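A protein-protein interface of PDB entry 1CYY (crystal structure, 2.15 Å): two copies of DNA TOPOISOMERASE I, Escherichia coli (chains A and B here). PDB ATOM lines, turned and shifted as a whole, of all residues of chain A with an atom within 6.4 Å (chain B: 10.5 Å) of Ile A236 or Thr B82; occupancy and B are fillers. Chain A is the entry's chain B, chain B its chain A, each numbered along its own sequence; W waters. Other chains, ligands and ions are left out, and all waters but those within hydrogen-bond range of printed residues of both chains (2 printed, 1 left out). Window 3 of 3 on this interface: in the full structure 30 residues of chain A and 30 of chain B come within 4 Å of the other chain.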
ATOM      1  N   ALA A  20      21.419  17.373  20.796  1.00  0.00           N
ATOM      2  CA  ALA A  20      20.709  17.289  22.059  1.00  0.00           C
ATOM      3  C   ALA A  20      20.818  15.890  22.653  1.00  0.00           C
ATOM      4  O   ALA A  20      20.712  14.888  21.940  1.00  0.00           O
ATOM      5  CB  ALA A  20      19.246  17.648  21.850  1.00  0.00           C
ATOM      6  N   ARG A  58      29.255   3.829  26.900  1.00  0.00           N
ATOM      7  CA  ARG A  58      28.233   3.723  25.876  1.00  0.00           C
ATOM      8  C   ARG A  58      28.055   2.250  25.550  1.00  0.00           C
ATOM      9  O   ARG A  58      29.015   1.551  25.244  1.00  0.00           O
ATOM     10  CB  ARG A  58      28.635   4.477  24.613  1.00  0.00           C
ATOM     11  CG  ARG A  58      27.604   4.357  23.509  1.00  0.00           C
ATOM     12  CD  ARG A  58      27.679   5.515  22.536  1.00  0.00           C
ATOM     13  NE  ARG A  58      26.463   5.610  21.735  1.00  0.00           N
ATOM     14  CZ  ARG A  58      25.969   6.746  21.251  1.00  0.00           C
ATOM     15  NH1 ARG A  58      24.851   6.737  20.529  1.00  0.00           N
ATOM     16  NH2 ARG A  58      26.588   7.897  21.491  1.00  0.00           N
ATOM     17  N   ASP A  60      25.615  -0.607  23.327  1.00  0.00           N
ATOM     18  CA  ASP A  60      24.632  -0.881  22.279  1.00  0.00           C
ATOM     19  C   ASP A  60      24.315  -2.373  22.248  1.00  0.00           C
ATOM     20  O   ASP A  60      25.209  -3.194  22.053  1.00  0.00           O
ATOM     21  CB  ASP A  60      25.173  -0.468  20.904  1.00  0.00           C
ATOM     22  CG  ASP A  60      24.939   0.993  20.599  1.00  0.00           C
ATOM     23  OD1 ASP A  60      24.214   1.284  19.616  1.00  0.00           O
ATOM     24  OD2 ASP A  60      25.477   1.849  21.342  1.00  0.00           O
ATOM     25  N   ASP A 196      17.026  -2.198  19.117  1.00  0.00           N
ATOM     26  CA  ASP A 196      18.455  -2.041  19.271  1.00  0.00           C
ATOM     27  C   ASP A 196      18.539  -0.889  20.270  1.00  0.00           C
ATOM     28  O   ASP A 196      18.197   0.253  19.952  1.00  0.00           O
ATOM     29  CB  ASP A 196      19.094  -1.727  17.925  1.00  0.00           C
ATOM     30  CG  ASP A 196      19.304  -2.991  17.095  1.00  0.00           C
ATOM     31  OD1 ASP A 196      20.135  -3.828  17.513  1.00  0.00           O
ATOM     32  OD2 ASP A 196      18.639  -3.167  16.053  1.00  0.00           O
ATOM     33  N   THR A 198      20.444   1.512  23.291  1.00  0.00           N
ATOM     34  CA  THR A 198      21.695   2.185  23.574  1.00  0.00           C
ATOM     35  C   THR A 198      21.575   2.744  24.978  1.00  0.00           C
ATOM     36  O   THR A 198      20.548   3.328  25.343  1.00  0.00           O
ATOM     37  CB  THR A 198      21.958   3.357  22.597  1.00  0.00           C
ATOM     38  OG1 THR A 198      21.973   2.872  21.251  1.00  0.00           O
ATOM     39  CG2 THR A 198      23.301   4.017  22.902  1.00  0.00           C
ATOM     40  N   GLY A 213      18.005   4.763  25.034  1.00  0.00           N
ATOM     41  CA  GLY A 213      17.317   4.979  23.783  1.00  0.00           C
ATOM     42  C   GLY A 213      17.162   3.641  23.107  1.00  0.00           C
ATOM     43  O   GLY A 213      17.880   2.702  23.419  1.00  0.00           O
ATOM     44  N   ARG A 214      16.202   3.526  22.208  1.00  0.00           N
ATOM     45  CA  ARG A 214      16.040   2.276  21.509  1.00  0.00           C
ATOM     46  C   ARG A 214      15.372   2.495  20.174  1.00  0.00           C
ATOM     47  O   ARG A 214      14.441   3.288  20.041  1.00  0.00           O
ATOM     48  CB  ARG A 214      15.258   1.270  22.348  1.00  0.00           C
ATOM     49  CG  ARG A 214      13.797   1.555  22.487  1.00  0.00           C
ATOM     50  CD  ARG A 214      13.145   0.411  23.233  1.00  0.00           C
ATOM     51  NE  ARG A 214      11.704   0.584  23.348  1.00  0.00           N
ATOM     52  CZ  ARG A 214      10.907  -0.237  24.027  1.00  0.00           C
ATOM     53  NH1 ARG A 214      11.415  -1.294  24.657  1.00  0.00           N
ATOM     54  NH2 ARG A 214       9.604   0.005  24.080  1.00  0.00           N
ATOM     55  N   ILE A 215      15.880   1.778  19.189  1.00  0.00           N
ATOM     56  CA  ILE A 215      15.403   1.829  17.823  1.00  0.00           C
ATOM     57  C   ILE A 215      14.604   0.563  17.527  1.00  0.00           C
ATOM     58  O   ILE A 215      15.103  -0.557  17.701  1.00  0.00           O
ATOM     59  CB  ILE A 215      16.610   1.909  16.862  1.00  0.00           C
ATOM     60  CG1 ILE A 215      17.339   3.239  17.071  1.00  0.00           C
ATOM     61  CG2 ILE A 215      16.165   1.721  15.427  1.00  0.00           C
ATOM     62  CD1 ILE A 215      18.669   3.341  16.332  1.00  0.00           C
ATOM     63  N   ASP A 234      13.696   4.777  23.232  1.00  0.00           N
ATOM     64  CA  ASP A 234      12.411   5.437  23.031  1.00  0.00           C
ATOM     65  C   ASP A 234      12.553   6.395  21.849  1.00  0.00           C
ATOM     66  O   ASP A 234      11.630   6.583  21.058  1.00  0.00           O
ATOM     67  CB  ASP A 234      12.035   6.222  24.284  1.00  0.00           C
ATOM     68  CG  ASP A 234      12.532   5.563  25.564  1.00  0.00           C
ATOM     69  OD1 ASP A 234      12.323   6.158  26.642  1.00  0.00           O
ATOM     70  OD2 ASP A 234      13.131   4.463  25.502  1.00  0.00           O
ATOM     71  N   ARG A 235      13.738   6.990  21.764  1.00  0.00           N
ATOM     72  CA  ARG A 235      14.122   7.935  20.723  1.00  0.00           C
ATOM     73  C   ARG A 235      15.541   7.526  20.327  1.00  0.00           C
ATOM     74  O   ARG A 235      16.077   6.551  20.858  1.00  0.00           O
ATOM     75  CB  ARG A 235      14.134   9.364  21.276  1.00  0.00           C
ATOM     76  CG  ARG A 235      15.174   9.614  22.388  1.00  0.00           C
ATOM     77  CD  ARG A 235      14.917   8.769  23.641  1.00  0.00           C
ATOM     78  NE  ARG A 235      15.932   8.956  24.682  1.00  0.00           N
ATOM     79  CZ  ARG A 235      16.105  10.076  25.385  1.00  0.00           C
ATOM     80  NH1 ARG A 235      15.325  11.130  25.167  1.00  0.00           N
ATOM     81  NH2 ARG A 235      17.060  10.142  26.310  1.00  0.00           N
ATOM     82  N   ILE A 236      16.163   8.261  19.411  1.00  0.00           N
ATOM     83  CA  ILE A 236      17.515   7.899  19.000  1.00  0.00           C
ATOM     84  C   ILE A 236      18.595   8.772  19.650  1.00  0.00           C
ATOM     85  O   ILE A 236      18.657   9.981  19.428  1.00  0.00           O
ATOM     86  CB  ILE A 236      17.633   7.904  17.437  1.00  0.00           C
ATOM     87  CG1 ILE A 236      19.099   7.963  17.007  1.00  0.00           C
ATOM     88  CG2 ILE A 236      16.823   9.023  16.845  1.00  0.00           C
ATOM     89  CD1 ILE A 236      19.857   6.689  17.285  1.00  0.00           C
ATOM     90  N   LEU A 237      19.432   8.147  20.478  1.00  0.00           N
ATOM     91  CA  LEU A 237      20.507   8.856  21.170  1.00  0.00           C
ATOM     92  C   LEU A 237      21.613   9.246  20.197  1.00  0.00           C
ATOM     93  O   LEU A 237      22.054   8.435  19.392  1.00  0.00           O
ATOM     94  CB  LEU A 237      21.101   7.989  22.282  1.00  0.00           C
ATOM     95  CG  LEU A 237      20.176   7.522  23.402  1.00  0.00           C
ATOM     96  CD1 LEU A 237      20.994   6.792  24.462  1.00  0.00           C
ATOM     97  CD2 LEU A 237      19.457   8.713  24.014  1.00  0.00           C
ATOM     98  N   PRO A 238      22.082  10.499  20.270  1.00  0.00           N
ATOM     99  CA  PRO A 238      23.142  10.969  19.379  1.00  0.00           C
ATOM    100  C   PRO A 238      24.481  10.300  19.654  1.00  0.00           C
ATOM    101  O   PRO A 238      24.739   9.831  20.759  1.00  0.00           O
ATOM    102  CB  PRO A 238      23.176  12.469  19.651  1.00  0.00           C
ATOM    103  CG  PRO A 238      22.824  12.542  21.099  1.00  0.00           C
ATOM    104  CD  PRO A 238      21.664  11.566  21.193  1.00  0.00           C
ATOM    105  N   PHE B  71      22.125   1.628  -0.152  1.00  0.00           N
ATOM    106  CA  PHE B  71      23.385   2.088   0.423  1.00  0.00           C
ATOM    107  C   PHE B  71      24.604   2.169  -0.478  1.00  0.00           C
ATOM    108  O   PHE B  71      24.711   1.481  -1.487  1.00  0.00           O
ATOM    109  CB  PHE B  71      23.791   1.209   1.607  1.00  0.00           C
ATOM    110  CG  PHE B  71      22.884   1.320   2.797  1.00  0.00           C
ATOM    111  CD1 PHE B  71      22.599   2.557   3.361  1.00  0.00           C
ATOM    112  CD2 PHE B  71      22.371   0.175   3.401  1.00  0.00           C
ATOM    113  CE1 PHE B  71      21.820   2.650   4.516  1.00  0.00           C
ATOM    114  CE2 PHE B  71      21.595   0.262   4.556  1.00  0.00           C
ATOM    115  CZ  PHE B  71      21.318   1.492   5.112  1.00  0.00           C
ATOM    116  N   SER B  74      29.430   5.387   2.222  1.00  0.00           N
ATOM    117  CA  SER B  74      29.163   6.428   3.209  1.00  0.00           C
ATOM    118  C   SER B  74      27.843   6.226   3.973  1.00  0.00           C
ATOM    119  O   SER B  74      27.813   6.255   5.210  1.00  0.00           O
ATOM    120  CB  SER B  74      29.143   7.797   2.525  1.00  0.00           C
ATOM    121  OG  SER B  74      28.144   7.827   1.521  1.00  0.00           O
ATOM    122  N   THR B  75      26.752   6.034   3.244  1.00  0.00           N
ATOM    123  CA  THR B  75      25.459   5.868   3.887  1.00  0.00           C
ATOM    124  C   THR B  75      25.346   4.575   4.709  1.00  0.00           C
ATOM    125  O   THR B  75      24.620   4.543   5.710  1.00  0.00           O
ATOM    126  CB  THR B  75      24.305   5.986   2.856  1.00  0.00           C
ATOM    127  OG1 THR B  75      24.539   5.100   1.754  1.00  0.00           O
ATOM    128  CG2 THR B  75      24.210   7.441   2.336  1.00  0.00           C
ATOM    129  N   LEU B  76      26.082   3.528   4.323  1.00  0.00           N
ATOM    130  CA  LEU B  76      26.051   2.282   5.084  1.00  0.00           C
ATOM    131  C   LEU B  76      26.751   2.503   6.422  1.00  0.00           C
ATOM    132  O   LEU B  76      26.300   2.002   7.454  1.00  0.00           O
ATOM    133  CB  LEU B  76      26.752   1.140   4.343  1.00  0.00           C
ATOM    134  CG  LEU B  76      26.939  -0.132   5.191  1.00  0.00           C
ATOM    135  CD1 LEU B  76      25.573  -0.710   5.563  1.00  0.00           C
ATOM    136  CD2 LEU B  76      27.762  -1.176   4.413  1.00  0.00           C
ATOM    137  N   GLN B  77      27.852   3.251   6.397  1.00  0.00           N
ATOM    138  CA  GLN B  77      28.609   3.534   7.610  1.00  0.00           C
ATOM    139  C   GLN B  77      27.784   4.388   8.582  1.00  0.00           C
ATOM    140  O   GLN B  77      27.812   4.169   9.789  1.00  0.00           O
ATOM    141  CB  GLN B  77      29.923   4.233   7.270  1.00  0.00           C
ATOM    142  CG  GLN B  77      30.901   3.379   6.461  1.00  0.00           C
ATOM    143  CD  GLN B  77      32.228   4.093   6.219  1.00  0.00           C
ATOM    144  OE1 GLN B  77      32.334   5.293   6.447  1.00  0.00           O
ATOM    145  NE2 GLN B  77      33.233   3.364   5.740  1.00  0.00           N
ATOM    146  N   GLN B  78      27.047   5.353   8.054  1.00  0.00           N
ATOM    147  CA  GLN B  78      26.197   6.191   8.887  1.00  0.00           C
ATOM    148  C   GLN B  78      25.028   5.377   9.468  1.00  0.00           C
ATOM    149  O   GLN B  78      24.728   5.490  10.657  1.00  0.00           O
ATOM    150  CB  GLN B  78      25.642   7.364   8.077  1.00  0.00           C
ATOM    151  CG  GLN B  78      26.709   8.311   7.549  1.00  0.00           C
ATOM    152  CD  GLN B  78      26.133   9.381   6.639  1.00  0.00           C
ATOM    153  OE1 GLN B  78      25.192  10.082   7.015  1.00  0.00           O
ATOM    154  NE2 GLN B  78      26.695   9.517   5.438  1.00  0.00           N
ATOM    155  N   ALA B  79      24.377   4.558   8.640  1.00  0.00           N
ATOM    156  CA  ALA B  79      23.239   3.764   9.108  1.00  0.00           C
ATOM    157  C   ALA B  79      23.650   2.679  10.107  1.00  0.00           C
ATOM    158  O   ALA B  79      22.943   2.436  11.070  1.00  0.00           O
ATOM    159  CB  ALA B  79      22.486   3.135   7.922  1.00  0.00           C
ATOM    160  N   ALA B  80      24.794   2.045   9.882  1.00  0.00           N
ATOM    161  CA  ALA B  80      25.259   0.991  10.778  1.00  0.00           C
ATOM    162  C   ALA B  80      25.596   1.590  12.140  1.00  0.00           C
ATOM    163  O   ALA B  80      25.382   0.954  13.178  1.00  0.00           O
ATOM    164  CB  ALA B  80      26.484   0.296  10.198  1.00  0.00           C
ATOM    165  N   SER B  81      26.143   2.804  12.125  1.00  0.00           N
ATOM    166  CA  SER B  81      26.496   3.479  13.358  1.00  0.00           C
ATOM    167  C   SER B  81      25.237   3.793  14.156  1.00  0.00           C
ATOM    168  O   SER B  81      25.146   3.458  15.333  1.00  0.00           O
ATOM    169  CB  SER B  81      27.232   4.789  13.077  1.00  0.00           C
ATOM    170  OG  SER B  81      27.231   5.579  14.251  1.00  0.00           O
ATOM    171  N   THR B  82      24.280   4.434  13.485  1.00  0.00           N
ATOM    172  CA  THR B  82      23.011   4.837  14.072  1.00  0.00           C
ATOM    173  C   THR B  82      22.105   3.685  14.501  1.00  0.00           C
ATOM    174  O   THR B  82      21.653   3.639  15.648  1.00  0.00           O
ATOM    175  CB  THR B  82      22.201   5.712  13.089  1.00  0.00           C
ATOM    176  OG1 THR B  82      22.926   6.910  12.814  1.00  0.00           O
ATOM    177  CG2 THR B  82      20.820   6.069  13.687  1.00  0.00           C
ATOM    178  N   ARG B  83      21.832   2.761  13.588  1.00  0.00           N
ATOM    179  CA  ARG B  83      20.945   1.652  13.911  1.00  0.00           C
ATOM    180  C   ARG B  83      21.576   0.500  14.676  1.00  0.00           C
ATOM    181  O   ARG B  83      20.921  -0.153  15.478  1.00  0.00           O
ATOM    182  CB  ARG B  83      20.294   1.112  12.639  1.00  0.00           C
ATOM    183  CG  ARG B  83      19.503   2.157  11.871  1.00  0.00           C
ATOM    184  CD  ARG B  83      18.489   1.509  10.952  1.00  0.00           C
ATOM    185  NE  ARG B  83      17.682   2.494  10.242  1.00  0.00           N
ATOM    186  CZ  ARG B  83      16.352   2.495  10.223  1.00  0.00           C
ATOM    187  NH1 ARG B  83      15.676   1.559  10.882  1.00  0.00           N
ATOM    188  NH2 ARG B  83      15.690   3.420   9.528  1.00  0.00           N
ATOM    189  N   LEU B  84      22.858   0.259  14.449  1.00  0.00           N
ATOM    190  CA  LEU B  84      23.513  -0.860  15.100  1.00  0.00           C
ATOM    191  C   LEU B  84      24.608  -0.506  16.090  1.00  0.00           C
ATOM    192  O   LEU B  84      25.037  -1.361  16.856  1.00  0.00           O
ATOM    193  CB  LEU B  84      24.067  -1.794  14.030  1.00  0.00           C
ATOM    194  CG  LEU B  84      23.025  -2.315  13.036  1.00  0.00           C
ATOM    195  CD1 LEU B  84      23.718  -3.237  12.045  1.00  0.00           C
ATOM    196  CD2 LEU B  84      21.904  -3.054  13.766  1.00  0.00           C
ATOM    197  N   GLY B  85      25.062   0.744  16.081  1.00  0.00           N
ATOM    198  CA  GLY B  85      26.125   1.143  16.989  1.00  0.00           C
ATOM    199  C   GLY B  85      27.505   0.699  16.532  1.00  0.00           C
ATOM    200  O   GLY B  85      28.450   0.706  17.316  1.00  0.00           O
ATOM    201  N   PHE B  86      27.629   0.312  15.263  1.00  0.00           N
ATOM    202  CA  PHE B  86      28.903  -0.147  14.706  1.00  0.00           C
ATOM    203  C   PHE B  86      29.785   1.008  14.250  1.00  0.00           C
ATOM    204  O   PHE B  86      29.332   1.905  13.549  1.00  0.00           O
ATOM    205  CB  PHE B  86      28.679  -1.052  13.484  1.00  0.00           C
ATOM    206  CG  PHE B  86      28.036  -2.377  13.790  1.00  0.00           C
ATOM    207  CD1 PHE B  86      27.695  -2.736  15.084  1.00  0.00           C
ATOM    208  CD2 PHE B  86      27.770  -3.269  12.759  1.00  0.00           C
ATOM    209  CE1 PHE B  86      27.094  -3.973  15.345  1.00  0.00           C
ATOM    210  CE2 PHE B  86      27.171  -4.504  13.009  1.00  0.00           C
ATOM    211  CZ  PHE B  86      26.833  -4.855  14.301  1.00  0.00           C
ATOM    212  N   GLY B  87      31.052   0.976  14.638  1.00  0.00           N
ATOM    213  CA  GLY B  87      31.962   2.017  14.203  1.00  0.00           C
ATOM    214  C   GLY B  87      32.332   1.762  12.752  1.00  0.00           C
ATOM    215  O   GLY B  87      31.947   0.743  12.186  1.00  0.00           O
ATOM    216  N   VAL B  88      33.089   2.670  12.150  1.00  0.00           N
ATOM    217  CA  VAL B  88      33.475   2.518  10.755  1.00  0.00           C
ATOM    218  C   VAL B  88      34.299   1.260  10.486  1.00  0.00           C
ATOM    219  O   VAL B  88      34.083   0.586   9.487  1.00  0.00           O
ATOM    220  CB  VAL B  88      34.240   3.765  10.276  1.00  0.00           C
ATOM    221  CG1 VAL B  88      34.893   3.508   8.929  1.00  0.00           C
ATOM    222  CG2 VAL B  88      33.275   4.923  10.176  1.00  0.00           C
ATOM    223  N   THR B  91      32.137  -1.920  10.653  1.00  0.00           N
ATOM    224  CA  THR B  91      31.228  -1.926   9.515  1.00  0.00           C
ATOM    225  C   THR B  91      31.896  -2.414   8.240  1.00  0.00           C
ATOM    226  O   THR B  91      31.363  -3.290   7.561  1.00  0.00           O
ATOM    227  CB  THR B  91      30.630  -0.527   9.267  1.00  0.00           C
ATOM    228  OG1 THR B  91      29.758  -0.181  10.351  1.00  0.00           O
ATOM    229  CG2 THR B  91      29.826  -0.510   7.969  1.00  0.00           C
ATOM    230  N   LEU B 177      24.297  -6.665   9.986  1.00  0.00           N
ATOM    231  CA  LEU B 177      24.653  -5.701   8.949  1.00  0.00           C
ATOM    232  C   LEU B 177      23.965  -6.114   7.650  1.00  0.00           C
ATOM    233  O   LEU B 177      23.475  -5.268   6.894  1.00  0.00           O
ATOM    234  CB  LEU B 177      26.166  -5.668   8.732  1.00  0.00           C
ATOM    235  CG  LEU B 177      26.633  -4.556   7.794  1.00  0.00           C
ATOM    236  CD1 LEU B 177      26.334  -3.221   8.455  1.00  0.00           C
ATOM    237  CD2 LEU B 177      28.136  -4.695   7.507  1.00  0.00           C
ATOM    238  N   LEU B 180      20.333  -5.105   7.650  1.00  0.00           N
ATOM    239  CA  LEU B 180      20.230  -3.671   7.430  1.00  0.00           C
ATOM    240  C   LEU B 180      20.371  -3.348   5.931  1.00  0.00           C
ATOM    241  O   LEU B 180      19.577  -2.598   5.371  1.00  0.00           O
ATOM    242  CB  LEU B 180      21.313  -2.935   8.228  1.00  0.00           C
ATOM    243  CG  LEU B 180      21.327  -1.414   8.033  1.00  0.00           C
ATOM    244  CD1 LEU B 180      20.002  -0.838   8.517  1.00  0.00           C
ATOM    245  CD2 LEU B 180      22.500  -0.790   8.781  1.00  0.00           C
ATOM    246  N   GLN B 184      17.201  -1.868   3.464  1.00  0.00           N
ATOM    247  CA  GLN B 184      17.338  -0.597   2.757  1.00  0.00           C
ATOM    248  C   GLN B 184      17.104  -0.827   1.263  1.00  0.00           C
ATOM    249  O   GLN B 184      16.426  -0.046   0.600  1.00  0.00           O
ATOM    250  CB  GLN B 184      18.744  -0.026   2.989  1.00  0.00           C
ATOM    251  CG  GLN B 184      19.002   1.354   2.393  1.00  0.00           C
ATOM    252  CD  GLN B 184      18.289   2.472   3.155  1.00  0.00           C
ATOM    253  OE1 GLN B 184      17.772   2.256   4.254  1.00  0.00           O
ATOM    254  NE2 GLN B 184      18.277   3.673   2.579  1.00  0.00           N
ATOM    255  N   MET B 225      11.431  -1.436   6.415  1.00  0.00           N
ATOM    256  CA  MET B 225      12.473  -0.655   7.078  1.00  0.00           C
ATOM    257  C   MET B 225      11.809   0.364   7.983  1.00  0.00           C
ATOM    258  O   MET B 225      11.329   1.393   7.514  1.00  0.00           O
ATOM    259  CB  MET B 225      13.343   0.081   6.057  1.00  0.00           C
ATOM    260  CG  MET B 225      14.405   1.004   6.662  1.00  0.00           C
ATOM    261  SD  MET B 225      15.980   0.196   7.086  1.00  0.00           S
ATOM    262  CE  MET B 225      15.482  -0.844   8.295  1.00  0.00           C
ATOM    263  N   PRO B 226      11.763   0.086   9.288  1.00  0.00           N
ATOM    264  CA  PRO B 226      11.146   1.009  10.243  1.00  0.00           C
ATOM    265  C   PRO B 226      11.790   2.383  10.120  1.00  0.00           C
ATOM    266  O   PRO B 226      13.011   2.494  10.084  1.00  0.00           O
ATOM    267  CB  PRO B 226      11.439   0.352  11.593  1.00  0.00           C
ATOM    268  CG  PRO B 226      11.460  -1.101  11.255  1.00  0.00           C
ATOM    269  CD  PRO B 226      12.275  -1.108   9.979  1.00  0.00           C
ATOM    270  N   ALA B 227      10.972   3.424  10.034  1.00  0.00           N
ATOM    271  CA  ALA B 227      11.490   4.784   9.918  1.00  0.00           C
ATOM    272  C   ALA B 227      12.029   5.244  11.265  1.00  0.00           C
ATOM    273  O   ALA B 227      11.431   4.979  12.302  1.00  0.00           O
ATOM    274  CB  ALA B 227      10.386   5.727   9.447  1.00  0.00           C
ATOM    275  N   LEU B 228      13.155   5.943  11.249  1.00  0.00           N
ATOM    276  CA  LEU B 228      13.750   6.427  12.483  1.00  0.00           C
ATOM    277  C   LEU B 228      12.875   7.482  13.159  1.00  0.00           C
ATOM    278  O   LEU B 228      12.858   8.645  12.746  1.00  0.00           O
ATOM    279  CB  LEU B 228      15.135   7.000  12.195  1.00  0.00           C
ATOM    280  CG  LEU B 228      16.153   5.973  11.711  1.00  0.00           C
ATOM    281  CD1 LEU B 228      17.437   6.673  11.303  1.00  0.00           C
ATOM    282  CD2 LEU B 228      16.414   4.965  12.814  1.00  0.00           C
ATOM    283  N   ASP B 234       7.756  14.451  12.308  1.00  0.00           N
ATOM    284  CA  ASP B 234       8.101  14.268  13.712  1.00  0.00           C
ATOM    285  C   ASP B 234       7.724  12.861  14.183  1.00  0.00           C
ATOM    286  O   ASP B 234       7.814  11.890  13.429  1.00  0.00           O
ATOM    287  CB  ASP B 234       7.381  15.325  14.563  1.00  0.00           C
ATOM    288  CG  ASP B 234       8.343  16.192  15.361  1.00  0.00           C
ATOM    289  OD1 ASP B 234       8.743  15.790  16.482  1.00  0.00           O
ATOM    290  OD2 ASP B 234       8.712  17.275  14.856  1.00  0.00           O
ATOM    291  N   ARG B 235       7.299  12.765  15.435  1.00  0.00           N
ATOM    292  CA  ARG B 235       6.907  11.502  16.040  1.00  0.00           C
ATOM    293  C   ARG B 235       5.579  10.977  15.501  1.00  0.00           C
ATOM    294  O   ARG B 235       4.743  11.746  15.033  1.00  0.00           O
ATOM    295  CB  ARG B 235       6.839  11.689  17.558  1.00  0.00           C
ATOM    296  CG  ARG B 235       6.953  13.160  18.001  1.00  0.00           C
ATOM    297  CD  ARG B 235       7.477  13.284  19.439  1.00  0.00           C
ATOM    298  NE  ARG B 235       6.750  12.398  20.344  1.00  0.00           N
ATOM    299  CZ  ARG B 235       5.442  12.485  20.558  1.00  0.00           C
ATOM    300  NH1 ARG B 235       4.739  13.423  19.935  1.00  0.00           N
ATOM    301  NH2 ARG B 235       4.834  11.625  21.365  1.00  0.00           N
HETATM  302  O   HOH W   1      18.410  -1.427  14.224  1.00  0.00           O
HETATM  303  O   HOH W   2      25.693   5.118  17.969  1.00  0.00           O
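2 positions are printed for both chains.
Of the 7 pairs that touch across the chains among the printed residues, none has its exchanged pair printed and touching as well.
Water W1 bridges OD2 of Asp A196 (2.5 Å) and O of Arg B83 (3.1 Å).
Water W2 lies within hydrogen-bond range of the guanidinium group (NH1) of Arg A58 (3.1 Å) and the backbone carbonyl oxygen (O) of Ser B81 (3.2 Å).
Of the 26 printed residues of chain B, 4 touch a printed residue of chain A.
Of the 13 printed residues of chain A, 4 touch a printed residue of chain B.
Hydrophobic or aromatic side chains of chain A that line the printed part of chain B: Ile A215 and Ile A236.
Along chain A the printed residues that touch a printed residue of chain B span positions 60 to 236.
Among the printed residues, 7 pairs touch across the chains.
Of the printed residues of chain B, Asp A60 touches Leu B84 (3.9 Å) and Gly B85 (3.3 Å).
Printed residues of chain B within 4 Å of Ile A215: Thr B82 (3.1 Å) and Arg B83 (3.7 Å).
Ile A236 touches just one residue of chain B: Thr B82.
No residue of chain B comes within 4 Å of Leu A237.
No residue of chain B comes within 4 Å of Pro A238.
Ser B81 touches none of the printed residues of chain A.
Of chain A, only Ile A215 and Ile A236 come within 4 Å of Thr B82.
Printed residues of chain A within 4 Å of Arg B83: Asp A196 (3.4 Å) and Ile A215 (3.7 Å).
Printed residues of chain A within 4 Å of Leu B84: Asp A60 and Asp A196.
Printed residues of chain A within 4 Å of Gly B85: Asp A60.
The nearest residue of chain A that does not touch Thr B82 is Asp A60 (5.3 Å).
The nearest printed residue of chain B that does not touch Asp A60 is Ser B81 (4.9 Å).
O of Ala B80 sits at hydrogen-bond distance from N of Gly B85.
The backbone carbonyl oxygen (O) of Gln B78 is in hydrogen-bond range of the side-chain hydroxyl (OG1) of Thr B82 (3.1 Å).
N of Ile A215 is in hydrogen-bond range of O of Asp A196 (2.9 Å).
OG1 of Thr A198 sits at hydrogen-bond distance from OD1 of Asp A60.
OD2 of Asp A60 lies within salt-bridge range of NE of Arg A58, at 3.9 Å.
The backbone carbonyl oxygen (O) of Pro B226 sits at hydrogen-bond distance from the guanidinium group (NH2) of Arg B83, 2.9 Å away.
Leu B84 touches Asp A60.
Asp A60 touches Gly B85.
Asp A196 touches Arg B83 (CB to O, 3.4 Å).
OD2 of Asp A196 touches CD2 of Leu B84, at 3.99 Å.
Ile A215 touches Thr B82 (CD1 to O, 3.1 Å).
Ile A215 touches Arg B83 (CD1 to CA, 3.7 Å).
Thr B82 touches Ile A236.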
